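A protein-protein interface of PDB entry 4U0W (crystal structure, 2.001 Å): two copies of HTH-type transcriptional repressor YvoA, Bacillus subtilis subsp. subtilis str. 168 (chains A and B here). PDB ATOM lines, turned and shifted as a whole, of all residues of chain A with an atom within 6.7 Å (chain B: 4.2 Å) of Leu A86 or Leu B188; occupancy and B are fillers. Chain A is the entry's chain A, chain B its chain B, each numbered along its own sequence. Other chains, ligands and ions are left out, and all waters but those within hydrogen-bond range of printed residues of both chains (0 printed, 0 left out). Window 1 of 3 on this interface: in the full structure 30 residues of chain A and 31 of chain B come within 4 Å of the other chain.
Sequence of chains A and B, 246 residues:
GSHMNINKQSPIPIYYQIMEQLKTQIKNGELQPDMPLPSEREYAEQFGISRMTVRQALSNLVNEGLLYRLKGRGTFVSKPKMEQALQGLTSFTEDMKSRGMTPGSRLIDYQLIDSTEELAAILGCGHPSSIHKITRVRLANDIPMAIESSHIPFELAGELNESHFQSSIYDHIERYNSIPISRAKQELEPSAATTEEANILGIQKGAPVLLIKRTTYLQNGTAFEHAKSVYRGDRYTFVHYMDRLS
Leu A86 touches Leu B188, but with the chains exchanged Leu A188 does not touch Leu B86 (4.2 Å).
Leu A86 touches His B240, and with the chains exchanged His A240 touches Leu B86.
Gln A186 touches His B240, and with the chains exchanged His A240 touches Gln B186.
Leu B188 touches its own counterpart, Leu A188.
Positions printed for both chains: 86, 186, 188, 212 and 240.
Of the 9 printed residues of chain B, 6 touch a printed residue of chain A.
Hydrophobic or aromatic side chains of chain B that line the printed part of chain A: Leu B86, Leu B188, His B240 and Met B242.
Hydrophobic or aromatic side chains of chain A within 4 Å of the printed part of chain B: Leu A86, Leu A188, Phe A238, Val A239 and His A240.
Along chain A the printed residues that touch a printed residue of chain B span positions 86 to 240.
Among the printed residues, no Asp or Glu carboxylate lies within 4 Å of a Lys or Arg side-chain nitrogen of the other chain.
The side-chain amide nitrogen (NE2) of Gln A186 sits at hydrogen-bond distance from a ring nitrogen (NE2) of His B240, at 2.9 Å.
A ring nitrogen (NE2) of His A240 sits at hydrogen-bond distance from the side-chain amide nitrogen (NE2) of Gln B186.
O of Leu A86 lies close to ND1 of His B240.
A ring nitrogen (ND1) of His A240 sits close to the backbone carbonyl oxygen (O) of Leu B86 (3.0 Å).
SD of Met B242 lies close to NH2 of Arg A214.
The backbone NH (N) of Leu B188 is in hydrogen-bond range of the backbone carbonyl oxygen (O) of Phe A238 (2.6 Å).
The backbone carbonyl oxygen (O) of Thr A237 lies within hydrogen-bond range of the backbone NH (N) of Gln A84 (2.9 Å).
The backbone NH (N) of Leu A86 lies within hydrogen-bond range of the backbone carbonyl oxygen (O) of Val A239 (2.8 Å).
The backbone NH (N) of Val A239 is in hydrogen-bond range of the backbone carbonyl oxygen (O) of Gln A84 (2.9 Å).
The side-chain amide oxygen of Gln A186 sits at hydrogen-bond distance from the guanidinium group of Arg A214 (2.8 Å).
Leu A86 touches just these residues of chain B: Leu B188, His B240 and Met B242.
Of the printed residues of chain B, Arg A214 touches Met B242.
Of the printed residues of chain B, Thr A237 touches Glu B187 (3.7 Å) and Leu B188 (3.9 Å).
Printed residues of chain B within 4 Å of Val A239: Gln B186 (3.3 Å) and Glu B187 (3.9 Å).
Printed residues of chain A within 4 Å of Gln B186: Phe A238, Val A239 and His A240.
Of the printed residues of chain A, Leu B188 touches Leu A86, Leu A188, Thr A237 and Phe A238.
The nearest printed residue of chain B that does not touch Leu A86 is Leu B86 (4.4 Å).
The nearest printed residue of chain A that does not touch His B240 is Leu A188 (4.01 Å).
Among the printed residues, merely in contact across the chains: Leu A86 with Leu B188 (3.95 Å), Leu A86 with Met B242 (3.0 Å), Gln A87 with Met B242 (3.5 Å), Gly A88 with Met B242 (3.5 Å), Leu A89 with Met B242 (3.997 Å), Gln A186 with Met B242 (3.7 Å), Leu A188 with Leu B188 (3.99 Å), Thr A237 with Glu B187 (3.7 Å), Thr A237 with Leu B188 (3.9 Å), Phe A238 with Gln B186 (3.6 Å), Phe A238 with Glu B187 (3.3 Å), Val A239 with Gln B186 (3.3 Å) and Val A239 with Glu B187 (3.9 Å).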
ATOM      1  N   GLN A  84      23.484 -13.101  -7.392  1.00  0.00           N
ATOM      2  CA  GLN A  84      23.200 -13.203  -8.801  1.00  0.00           C
ATOM      3  C   GLN A  84      24.087 -14.291  -9.387  1.00  0.00           C
ATOM      4  O   GLN A  84      25.304 -14.144  -9.409  1.00  0.00           O
ATOM      5  CB  GLN A  84      23.458 -11.851  -9.486  1.00  0.00           C
ATOM      6  CG  GLN A  84      23.107 -11.792 -10.956  1.00  0.00           C
ATOM      7  CD  GLN A  84      21.612 -11.798 -11.191  1.00  0.00           C
ATOM      8  OE1 GLN A  84      20.858 -11.173 -10.448  1.00  0.00           O
ATOM      9  NE2 GLN A  84      21.178 -12.483 -12.250  1.00  0.00           N
ATOM     10  N   ALA A  85      23.484 -15.385  -9.840  1.00  0.00           N
ATOM     11  CA  ALA A  85      24.212 -16.437 -10.544  1.00  0.00           C
ATOM     12  C   ALA A  85      24.595 -15.999 -11.961  1.00  0.00           C
ATOM     13  O   ALA A  85      23.734 -15.832 -12.820  1.00  0.00           O
ATOM     14  CB  ALA A  85      23.377 -17.713 -10.596  1.00  0.00           C
ATOM     15  N   LEU A  86      25.889 -15.848 -12.215  1.00  0.00           N
ATOM     16  CA  LEU A  86      26.346 -15.341 -13.512  1.00  0.00           C
ATOM     17  C   LEU A  86      26.247 -16.348 -14.658  1.00  0.00           C
ATOM     18  O   LEU A  86      26.220 -15.957 -15.819  1.00  0.00           O
ATOM     19  CB  LEU A  86      27.789 -14.859 -13.400  1.00  0.00           C
ATOM     20  CG  LEU A  86      27.997 -13.604 -12.558  1.00  0.00           C
ATOM     21  CD1 LEU A  86      29.468 -13.314 -12.427  1.00  0.00           C
ATOM     22  CD2 LEU A  86      27.294 -12.413 -13.196  1.00  0.00           C
ATOM     23  N   GLN A  87      26.207 -17.641 -14.358  1.00  0.00           N
ATOM     24  CA  GLN A  87      26.275 -18.624 -15.442  1.00  0.00           C
ATOM     25  C   GLN A  87      24.917 -19.009 -16.051  1.00  0.00           C
ATOM     26  O   GLN A  87      24.867 -19.613 -17.119  1.00  0.00           O
ATOM     27  CB  GLN A  87      27.006 -19.867 -14.945  1.00  0.00           C
ATOM     28  CG  GLN A  87      28.521 -19.663 -14.883  1.00  0.00           C
ATOM     29  CD  GLN A  87      29.194 -20.577 -13.880  1.00  0.00           C
ATOM     30  OE1 GLN A  87      28.834 -20.592 -12.698  1.00  0.00           O
ATOM     31  NE2 GLN A  87      30.169 -21.350 -14.341  1.00  0.00           N
ATOM     32  N   GLY A  88      23.828 -18.659 -15.376  1.00  0.00           N
ATOM     33  CA  GLY A  88      22.495 -18.964 -15.865  1.00  0.00           C
ATOM     34  C   GLY A  88      21.856 -17.774 -16.568  1.00  0.00           C
ATOM     35  O   GLY A  88      21.668 -16.701 -15.979  1.00  0.00           O
ATOM     36  N   LEU A  89      21.534 -17.961 -17.843  1.00  0.00           N
ATOM     37  CA  LEU A  89      20.897 -16.911 -18.628  1.00  0.00           C
ATOM     38  C   LEU A  89      19.441 -16.706 -18.184  1.00  0.00           C
ATOM     39  O   LEU A  89      18.571 -17.544 -18.434  1.00  0.00           O
ATOM     40  CB  LEU A  89      20.965 -17.251 -20.118  1.00  0.00           C
ATOM     41  CG  LEU A  89      20.282 -16.239 -21.045  1.00  0.00           C
ATOM     42  CD1 LEU A  89      20.689 -14.823 -20.678  1.00  0.00           C
ATOM     43  CD2 LEU A  89      20.622 -16.544 -22.504  1.00  0.00           C
ATOM     44  N   GLN A 186      28.728 -11.832 -21.413  1.00  0.00           N
ATOM     45  CA  GLN A 186      28.696 -10.651 -20.533  1.00  0.00           C
ATOM     46  C   GLN A 186      30.101 -10.154 -20.194  1.00  0.00           C
ATOM     47  O   GLN A 186      31.013 -10.954 -20.019  1.00  0.00           O
ATOM     48  CB  GLN A 186      27.940 -10.939 -19.229  1.00  0.00           C
ATOM     49  CG  GLN A 186      26.486 -10.544 -19.271  1.00  0.00           C
ATOM     50  CD  GLN A 186      25.777 -10.623 -17.932  1.00  0.00           C
ATOM     51  OE1 GLN A 186      24.641 -10.169 -17.812  1.00  0.00           O
ATOM     52  NE2 GLN A 186      26.433 -11.202 -16.914  1.00  0.00           N
ATOM     53  N   LEU A 188      32.059  -7.573 -17.424  1.00  0.00           N
ATOM     54  CA  LEU A 188      31.856  -6.939 -16.128  1.00  0.00           C
ATOM     55  C   LEU A 188      32.983  -5.964 -15.813  1.00  0.00           C
ATOM     56  O   LEU A 188      34.148  -6.277 -16.002  1.00  0.00           O
ATOM     57  CB  LEU A 188      31.767  -7.998 -14.999  1.00  0.00           C
ATOM     58  CG  LEU A 188      30.868  -9.216 -15.253  1.00  0.00           C
ATOM     59  CD1 LEU A 188      30.867 -10.211 -14.079  1.00  0.00           C
ATOM     60  CD2 LEU A 188      29.450  -8.784 -15.579  1.00  0.00           C
ATOM     61  N   LEU A 210      28.299  -2.324 -10.497  1.00  0.00           N
ATOM     62  CA  LEU A 210      28.855  -3.193 -11.504  1.00  0.00           C
ATOM     63  C   LEU A 210      28.326  -2.781 -12.892  1.00  0.00           C
ATOM     64  O   LEU A 210      27.119  -2.786 -13.132  1.00  0.00           O
ATOM     65  CB  LEU A 210      28.520  -4.645 -11.233  1.00  0.00           C
ATOM     66  CG  LEU A 210      29.448  -5.568 -12.019  1.00  0.00           C
ATOM     67  CD1 LEU A 210      30.900  -5.315 -11.560  1.00  0.00           C
ATOM     68  CD2 LEU A 210      29.033  -7.018 -11.821  1.00  0.00           C
ATOM     69  N   ILE A 212      27.767  -3.685 -16.577  1.00  0.00           N
ATOM     70  CA  ILE A 212      27.593  -4.946 -17.261  1.00  0.00           C
ATOM     71  C   ILE A 212      27.239  -4.695 -18.727  1.00  0.00           C
ATOM     72  O   ILE A 212      26.352  -3.911 -19.017  1.00  0.00           O
ATOM     73  CB  ILE A 212      26.501  -5.813 -16.599  1.00  0.00           C
ATOM     74  CG1 ILE A 212      26.794  -5.966 -15.096  1.00  0.00           C
ATOM     75  CG2 ILE A 212      26.445  -7.172 -17.285  1.00  0.00           C
ATOM     76  CD1 ILE A 212      25.734  -6.779 -14.291  1.00  0.00           C
ATOM     77  N   ARG A 214      25.984  -6.926 -21.955  1.00  0.00           N
ATOM     78  CA  ARG A 214      25.473  -8.243 -22.348  1.00  0.00           C
ATOM     79  C   ARG A 214      25.057  -8.334 -23.824  1.00  0.00           C
ATOM     80  O   ARG A 214      24.292  -7.508 -24.306  1.00  0.00           O
ATOM     81  CB  ARG A 214      24.270  -8.625 -21.479  1.00  0.00           C
ATOM     82  CG  ARG A 214      23.611  -9.932 -21.917  1.00  0.00           C
ATOM     83  CD  ARG A 214      22.371 -10.287 -21.097  1.00  0.00           C
ATOM     84  NE  ARG A 214      22.679 -10.615 -19.699  1.00  0.00           N
ATOM     85  CZ  ARG A 214      21.809 -11.148 -18.845  1.00  0.00           C
ATOM     86  NH1 ARG A 214      20.577 -11.431 -19.242  1.00  0.00           N
ATOM     87  NH2 ARG A 214      22.168 -11.409 -17.587  1.00  0.00           N
ATOM     88  N   TYR A 236      23.957  -6.426  -4.157  1.00  0.00           N
ATOM     89  CA  TYR A 236      24.270  -7.573  -4.998  1.00  0.00           C
ATOM     90  C   TYR A 236      25.634  -8.204  -4.693  1.00  0.00           C
ATOM     91  O   TYR A 236      26.623  -7.510  -4.475  1.00  0.00           O
ATOM     92  CB  TYR A 236      24.265  -7.166  -6.480  1.00  0.00           C
ATOM     93  CG  TYR A 236      22.916  -7.164  -7.161  1.00  0.00           C
ATOM     94  CD1 TYR A 236      22.362  -8.341  -7.643  1.00  0.00           C
ATOM     95  CD2 TYR A 236      22.216  -5.977  -7.361  1.00  0.00           C
ATOM     96  CE1 TYR A 236      21.125  -8.346  -8.285  1.00  0.00           C
ATOM     97  CE2 TYR A 236      20.980  -5.971  -8.007  1.00  0.00           C
ATOM     98  CZ  TYR A 236      20.448  -7.157  -8.470  1.00  0.00           C
ATOM     99  OH  TYR A 236      19.225  -7.163  -9.101  1.00  0.00           O
ATOM    100  N   THR A 237      25.680  -9.525  -4.754  1.00  0.00           N
ATOM    101  CA  THR A 237      26.924 -10.248  -4.853  1.00  0.00           C
ATOM    102  C   THR A 237      26.854 -11.132  -6.095  1.00  0.00           C
ATOM    103  O   THR A 237      25.874 -11.846  -6.292  1.00  0.00           O
ATOM    104  CB  THR A 237      27.177 -11.104  -3.590  1.00  0.00           C
ATOM    105  OG1 THR A 237      27.476 -10.238  -2.485  1.00  0.00           O
ATOM    106  CG2 THR A 237      28.342 -12.033  -3.814  1.00  0.00           C
ATOM    107  N   PHE A 238      27.873 -11.090  -6.944  1.00  0.00           N
ATOM    108  CA  PHE A 238      27.824 -11.886  -8.160  1.00  0.00           C
ATOM    109  C   PHE A 238      28.644 -13.155  -8.021  1.00  0.00           C
ATOM    110  O   PHE A 238      29.827 -13.107  -7.689  1.00  0.00           O
ATOM    111  CB  PHE A 238      28.289 -11.044  -9.356  1.00  0.00           C
ATOM    112  CG  PHE A 238      27.488  -9.794  -9.521  1.00  0.00           C
ATOM    113  CD1 PHE A 238      27.765  -8.673  -8.760  1.00  0.00           C
ATOM    114  CD2 PHE A 238      26.406  -9.762 -10.387  1.00  0.00           C
ATOM    115  CE1 PHE A 238      26.992  -7.535  -8.869  1.00  0.00           C
ATOM    116  CE2 PHE A 238      25.637  -8.622 -10.509  1.00  0.00           C
ATOM    117  CZ  PHE A 238      25.926  -7.512  -9.755  1.00  0.00           C
ATOM    118  N   VAL A 239      28.000 -14.285  -8.301  1.00  0.00           N
ATOM    119  CA  VAL A 239      28.578 -15.601  -8.068  1.00  0.00           C
ATOM    120  C   VAL A 239      28.691 -16.419  -9.344  1.00  0.00           C
ATOM    121  O   VAL A 239      27.787 -16.428 -10.176  1.00  0.00           O
ATOM    122  CB  VAL A 239      27.735 -16.389  -7.035  1.00  0.00           C
ATOM    123  CG1 VAL A 239      28.404 -17.700  -6.662  1.00  0.00           C
ATOM    124  CG2 VAL A 239      27.521 -15.548  -5.801  1.00  0.00           C
ATOM    125  N   HIS A 240      29.821 -17.096  -9.498  1.00  0.00           N
ATOM    126  CA  HIS A 240      30.011 -18.040 -10.585  1.00  0.00           C
ATOM    127  C   HIS A 240      30.960 -19.139 -10.126  1.00  0.00           C
ATOM    128  O   HIS A 240      31.597 -19.021  -9.075  1.00  0.00           O
ATOM    129  CB  HIS A 240      30.560 -17.336 -11.817  1.00  0.00           C
ATOM    130  CG  HIS A 240      31.962 -16.860 -11.639  1.00  0.00           C
ATOM    131  ND1 HIS A 240      33.051 -17.544 -12.137  1.00  0.00           N
ATOM    132  CD2 HIS A 240      32.459 -15.796 -10.965  1.00  0.00           C
ATOM    133  CE1 HIS A 240      34.159 -16.907 -11.798  1.00  0.00           C
ATOM    134  NE2 HIS A 240      33.826 -15.842 -11.087  1.00  0.00           N
ATOM    135  N   LEU B  86      36.320 -15.852 -16.978  1.00  0.00           N
ATOM    136  CA  LEU B  86      35.810 -16.192 -15.653  1.00  0.00           C
ATOM    137  C   LEU B  86      35.379 -17.633 -15.464  1.00  0.00           C
ATOM    138  O   LEU B  86      34.945 -17.981 -14.374  1.00  0.00           O
ATOM    139  CB  LEU B  86      34.615 -15.312 -15.295  1.00  0.00           C
ATOM    140  CG  LEU B  86      34.825 -13.953 -14.652  1.00  0.00           C
ATOM    141  CD1 LEU B  86      33.477 -13.462 -14.219  1.00  0.00           C
ATOM    142  CD2 LEU B  86      35.763 -14.053 -13.465  1.00  0.00           C
ATOM    143  N   GLN B 186      33.446 -18.364  -6.872  1.00  0.00           N
ATOM    144  CA  GLN B 186      33.905 -16.983  -6.776  1.00  0.00           C
ATOM    145  C   GLN B 186      32.753 -15.994  -6.547  1.00  0.00           C
ATOM    146  O   GLN B 186      31.700 -16.094  -7.172  1.00  0.00           O
ATOM    147  CB  GLN B 186      34.704 -16.617  -8.042  1.00  0.00           C
ATOM    148  CG  GLN B 186      35.992 -15.906  -7.746  1.00  0.00           C
ATOM    149  CD  GLN B 186      36.931 -15.771  -8.935  1.00  0.00           C
ATOM    150  OE1 GLN B 186      38.118 -16.097  -8.834  1.00  0.00           O
ATOM    151  NE2 GLN B 186      36.418 -15.259 -10.055  1.00  0.00           N
ATOM    152  N   GLU B 187      32.957 -15.042  -5.636  1.00  0.00           N
ATOM    153  CA  GLU B 187      31.974 -13.998  -5.365  1.00  0.00           C
ATOM    154  C   GLU B 187      32.555 -12.646  -5.720  1.00  0.00           C
ATOM    155  O   GLU B 187      33.615 -12.268  -5.221  1.00  0.00           O
ATOM    156  CB  GLU B 187      31.523 -13.995  -3.892  1.00  0.00           C
ATOM    157  CG  GLU B 187      30.663 -15.176  -3.485  1.00  0.00           C
ATOM    158  CD  GLU B 187      30.464 -15.281  -1.959  1.00  0.00           C
ATOM    159  OE1 GLU B 187      30.326 -14.244  -1.271  1.00  0.00           O
ATOM    160  OE2 GLU B 187      30.450 -16.417  -1.448  1.00  0.00           O
ATOM    161  N   LEU B 188      31.849 -11.905  -6.568  1.00  0.00           N
ATOM    162  CA  LEU B 188      32.372 -10.649  -7.095  1.00  0.00           C
ATOM    163  C   LEU B 188      31.589  -9.491  -6.542  1.00  0.00           C
ATOM    164  O   LEU B 188      30.363  -9.540  -6.456  1.00  0.00           O
ATOM    165  CB  LEU B 188      32.313 -10.629  -8.635  1.00  0.00           C
ATOM    166  CG  LEU B 188      32.824 -11.864  -9.356  1.00  0.00           C
ATOM    167  CD1 LEU B 188      32.733 -11.707 -10.887  1.00  0.00           C
ATOM    168  CD2 LEU B 188      34.244 -12.176  -8.921  1.00  0.00           C
ATOM    169  N   GLU B 189      32.295  -8.427  -6.204  1.00  0.00           N
ATOM    170  CA  GLU B 189      31.664  -7.237  -5.668  1.00  0.00           C
ATOM    171  C   GLU B 189      32.435  -5.994  -6.126  1.00  0.00           C
ATOM    172  O   GLU B 189      33.655  -5.942  -5.990  1.00  0.00           O
ATOM    173  CB  GLU B 189      31.619  -7.336  -4.137  1.00  0.00           C
ATOM    174  CG  GLU B 189      30.774  -6.302  -3.464  1.00  0.00           C
ATOM    175  CD  GLU B 189      30.693  -6.505  -1.961  1.00  0.00           C
ATOM    176  OE1 GLU B 189      30.630  -5.481  -1.239  1.00  0.00           O
ATOM    177  OE2 GLU B 189      30.691  -7.679  -1.513  1.00  0.00           O
ATOM    178  N   LEU B 211      36.191  -6.473  -5.912  1.00  0.00           N
ATOM    179  CA  LEU B 211      36.448  -7.286  -4.718  1.00  0.00           C
ATOM    180  C   LEU B 211      36.075  -8.734  -4.974  1.00  0.00           C
ATOM    181  O   LEU B 211      34.916  -9.041  -5.214  1.00  0.00           O
ATOM    182  CB  LEU B 211      35.648  -6.739  -3.533  1.00  0.00           C
ATOM    183  CG  LEU B 211      36.440  -6.006  -2.466  1.00  0.00           C
ATOM    184  CD1 LEU B 211      35.484  -5.323  -1.488  1.00  0.00           C
ATOM    185  CD2 LEU B 211      37.328  -7.022  -1.738  1.00  0.00           C
ATOM    186  N   ILE B 212      37.049  -9.634  -4.932  1.00  0.00           N
ATOM    187  CA  ILE B 212      36.780 -11.009  -5.298  1.00  0.00           C
ATOM    188  C   ILE B 212      37.057 -11.983  -4.143  1.00  0.00           C
ATOM    189  O   ILE B 212      38.130 -11.943  -3.541  1.00  0.00           O
ATOM    190  CB  ILE B 212      37.616 -11.419  -6.512  1.00  0.00           C
ATOM    191  CG1 ILE B 212      37.414 -10.412  -7.666  1.00  0.00           C
ATOM    192  CG2 ILE B 212      37.269 -12.842  -6.912  1.00  0.00           C
ATOM    193  CD1 ILE B 212      38.185 -10.770  -8.921  1.00  0.00           C
ATOM    194  N   HIS B 240      32.493 -13.491 -19.134  1.00  0.00           N
ATOM    195  CA  HIS B 240      31.957 -14.839 -18.994  1.00  0.00           C
ATOM    196  C   HIS B 240      30.797 -15.071 -19.953  1.00  0.00           C
ATOM    197  O   HIS B 240      30.275 -14.130 -20.556  1.00  0.00           O
ATOM    198  CB  HIS B 240      31.504 -15.085 -17.565  1.00  0.00           C
ATOM    199  CG  HIS B 240      30.282 -14.316 -17.200  1.00  0.00           C
ATOM    200  ND1 HIS B 240      29.021 -14.868 -17.228  1.00  0.00           N
ATOM    201  CD2 HIS B 240      30.122 -13.022 -16.836  1.00  0.00           C
ATOM    202  CE1 HIS B 240      28.135 -13.953 -16.873  1.00  0.00           C
ATOM    203  NE2 HIS B 240      28.777 -12.823 -16.636  1.00  0.00           N
ATOM    204  N   MET B 242      26.988 -17.234 -20.659  1.00  0.00           N
ATOM    205  CA  MET B 242      25.830 -17.751 -19.948  1.00  0.00           C
ATOM    206  C   MET B 242      25.037 -18.671 -20.860  1.00  0.00           C
ATOM    207  O   MET B 242      25.007 -18.478 -22.087  1.00  0.00           O
ATOM    208  CB  MET B 242      24.935 -16.616 -19.456  1.00  0.00           C
ATOM    209  CG  MET B 242      25.614 -15.258 -19.355  1.00  0.00           C
ATOM    210  SD  MET B 242      24.421 -13.979 -18.893  1.00  0.00           S
ATOM    211  CE  MET B 242      24.062 -14.409 -17.204  1.00  0.00           C
